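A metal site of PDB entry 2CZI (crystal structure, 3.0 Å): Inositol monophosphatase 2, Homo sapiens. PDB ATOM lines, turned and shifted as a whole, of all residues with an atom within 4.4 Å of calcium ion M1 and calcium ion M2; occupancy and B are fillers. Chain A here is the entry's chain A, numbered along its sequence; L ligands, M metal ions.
Calcium ion M1 is bound by the side-chain carboxylate of Glu 92 (2.0 Å), the backbone carbonyl oxygen of Ile 114 (2.1 Å), an oxygen (O2) of the ligand (2.3 Å), the side-chain carboxylate of Asp 112 (2.4 Å) and an oxygen (O3) of the ligand (2.8 Å).
Within 4 Å of calcium ion M2: Asp 112, Asp 115 and Asp 242.
Of the 7 residues printed, 4 come within 4 Å of calcium ion M1.
The nearest printed residue that does not touch calcium ion M1 is Asp 69 (4.3 Å).
Calcium ion M2 is bound by O2 of the ligand, 2.3 Å away.
Calcium ion M2 is bound by OD1 of Asp 242, 2.5 Å away.
Calcium ion M2 is bound by the side-chain carboxylate (OD1) of Asp 112, at 2.6 Å.
The side-chain carboxylate (OD2) of Asp 115 binds calcium ion M2 (2.7 Å).
Calcium ion M2 has four donor atoms within binding distance.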
ATOM      1  N   ASP A  69      17.588  -0.844  -4.629  1.00  0.00           N
ATOM      2  CA  ASP A  69      18.721  -0.914  -3.697  1.00  0.00           C
ATOM      3  C   ASP A  69      18.370  -0.172  -2.425  1.00  0.00           C
ATOM      4  O   ASP A  69      18.654  -0.641  -1.332  1.00  0.00           O
ATOM      5  CB  ASP A  69      19.976  -0.314  -4.342  1.00  0.00           C
ATOM      6  CG  ASP A  69      21.238  -0.657  -3.566  1.00  0.00           C
ATOM      7  OD1 ASP A  69      22.312  -0.857  -4.156  1.00  0.00           O
ATOM      8  OD2 ASP A  69      21.146  -0.732  -2.329  1.00  0.00           O
ATOM      9  N   GLU A  92      26.364  -0.387   1.563  1.00  0.00           N
ATOM     10  CA  GLU A  92      26.811   0.498   0.492  1.00  0.00           C
ATOM     11  C   GLU A  92      26.374   1.962   0.595  1.00  0.00           C
ATOM     12  O   GLU A  92      27.133   2.875   0.238  1.00  0.00           O
ATOM     13  CB  GLU A  92      26.432  -0.063  -0.875  1.00  0.00           C
ATOM     14  CG  GLU A  92      27.665  -0.620  -1.547  1.00  0.00           C
ATOM     15  CD  GLU A  92      27.414  -0.854  -3.004  1.00  0.00           C
ATOM     16  OE1 GLU A  92      26.653  -1.788  -3.292  1.00  0.00           O
ATOM     17  OE2 GLU A  92      27.944  -0.090  -3.865  1.00  0.00           O
ATOM     18  N   ASP A 112      25.227  -5.671   2.064  1.00  0.00           N
ATOM     19  CA  ASP A 112      25.347  -5.183   0.705  1.00  0.00           C
ATOM     20  C   ASP A 112      23.958  -5.540   0.141  1.00  0.00           C
ATOM     21  O   ASP A 112      23.751  -6.604  -0.425  1.00  0.00           O
ATOM     22  CB  ASP A 112      26.458  -5.923  -0.027  1.00  0.00           C
ATOM     23  CG  ASP A 112      26.762  -5.309  -1.360  1.00  0.00           C
ATOM     24  OD1 ASP A 112      27.730  -5.730  -2.007  1.00  0.00           O
ATOM     25  OD2 ASP A 112      26.020  -4.386  -1.749  1.00  0.00           O
ATOM     26  N   ILE A 114      22.358  -5.057  -2.401  1.00  0.00           N
ATOM     27  CA  ILE A 114      22.321  -5.612  -3.736  1.00  0.00           C
ATOM     28  C   ILE A 114      23.720  -5.667  -4.323  1.00  0.00           C
ATOM     29  O   ILE A 114      24.231  -4.631  -4.678  1.00  0.00           O
ATOM     30  CB  ILE A 114      21.464  -4.737  -4.694  1.00  0.00           C
ATOM     31  CG1 ILE A 114      20.016  -4.710  -4.209  1.00  0.00           C
ATOM     32  CG2 ILE A 114      21.573  -5.253  -6.151  1.00  0.00           C
ATOM     33  CD1 ILE A 114      19.038  -4.094  -5.184  1.00  0.00           C
ATOM     34  N   ASP A 115      24.317  -6.851  -4.420  1.00  0.00           N
ATOM     35  CA  ASP A 115      25.666  -7.005  -4.993  1.00  0.00           C
ATOM     36  C   ASP A 115      25.503  -7.330  -6.472  1.00  0.00           C
ATOM     37  O   ASP A 115      25.058  -8.426  -6.828  1.00  0.00           O
ATOM     38  CB  ASP A 115      26.416  -8.154  -4.303  1.00  0.00           C
ATOM     39  CG  ASP A 115      27.804  -8.375  -4.892  1.00  0.00           C
ATOM     40  OD1 ASP A 115      28.142  -9.531  -5.229  1.00  0.00           O
ATOM     41  OD2 ASP A 115      28.578  -7.407  -4.998  1.00  0.00           O
ATOM     42  N   TRP A 241      31.760  -4.967   3.005  1.00  0.00           N
ATOM     43  CA  TRP A 241      30.435  -5.564   2.985  1.00  0.00           C
ATOM     44  C   TRP A 241      30.278  -6.648   1.934  1.00  0.00           C
ATOM     45  O   TRP A 241      29.244  -7.288   1.862  1.00  0.00           O
ATOM     46  CB  TRP A 241      29.368  -4.496   2.776  1.00  0.00           C
ATOM     47  CG  TRP A 241      29.645  -3.610   1.622  1.00  0.00           C
ATOM     48  CD1 TRP A 241      29.615  -3.932   0.312  1.00  0.00           C
ATOM     49  CD2 TRP A 241      29.997  -2.224   1.690  1.00  0.00           C
ATOM     50  NE1 TRP A 241      29.925  -2.840  -0.459  1.00  0.00           N
ATOM     51  CE2 TRP A 241      30.169  -1.774   0.365  1.00  0.00           C
ATOM     52  CE3 TRP A 241      30.194  -1.319   2.746  1.00  0.00           C
ATOM     53  CZ2 TRP A 241      30.527  -0.460   0.064  1.00  0.00           C
ATOM     54  CZ3 TRP A 241      30.546  -0.013   2.446  1.00  0.00           C
ATOM     55  CH2 TRP A 241      30.710   0.405   1.102  1.00  0.00           C
ATOM     56  N   ASP A 242      31.308  -6.855   1.122  1.00  0.00           N
ATOM     57  CA  ASP A 242      31.240  -7.881   0.095  1.00  0.00           C
ATOM     58  C   ASP A 242      31.713  -9.199   0.650  1.00  0.00           C
ATOM     59  O   ASP A 242      31.013 -10.213   0.583  1.00  0.00           O
ATOM     60  CB  ASP A 242      32.126  -7.525  -1.089  1.00  0.00           C
ATOM     61  CG  ASP A 242      31.610  -6.340  -1.873  1.00  0.00           C
ATOM     62  OD1 ASP A 242      30.395  -6.311  -2.153  1.00  0.00           O
ATOM     63  OD2 ASP A 242      32.426  -5.457  -2.219  1.00  0.00           O
HETATM   64  P1  LIG L   1      27.456  -3.211  -6.524  1.00  0.00           P
HETATM   65  O1  LIG L   1      28.542  -2.175  -6.543  1.00  0.00           O
HETATM   66  O2  LIG L   1      27.561  -4.032  -5.281  1.00  0.00           O
HETATM   67  O3  LIG L   1      26.108  -2.554  -6.544  1.00  0.00           O
HETATM   68  O4  LIG L   1      27.575  -4.117  -7.722  1.00  0.00           O
HETATM   69 CA    CA M   1      25.770  -3.422  -3.920  1.00  0.00          CA
HETATM   70 CA    CA M   2      29.224  -4.966  -3.938  1.00  0.00          CA
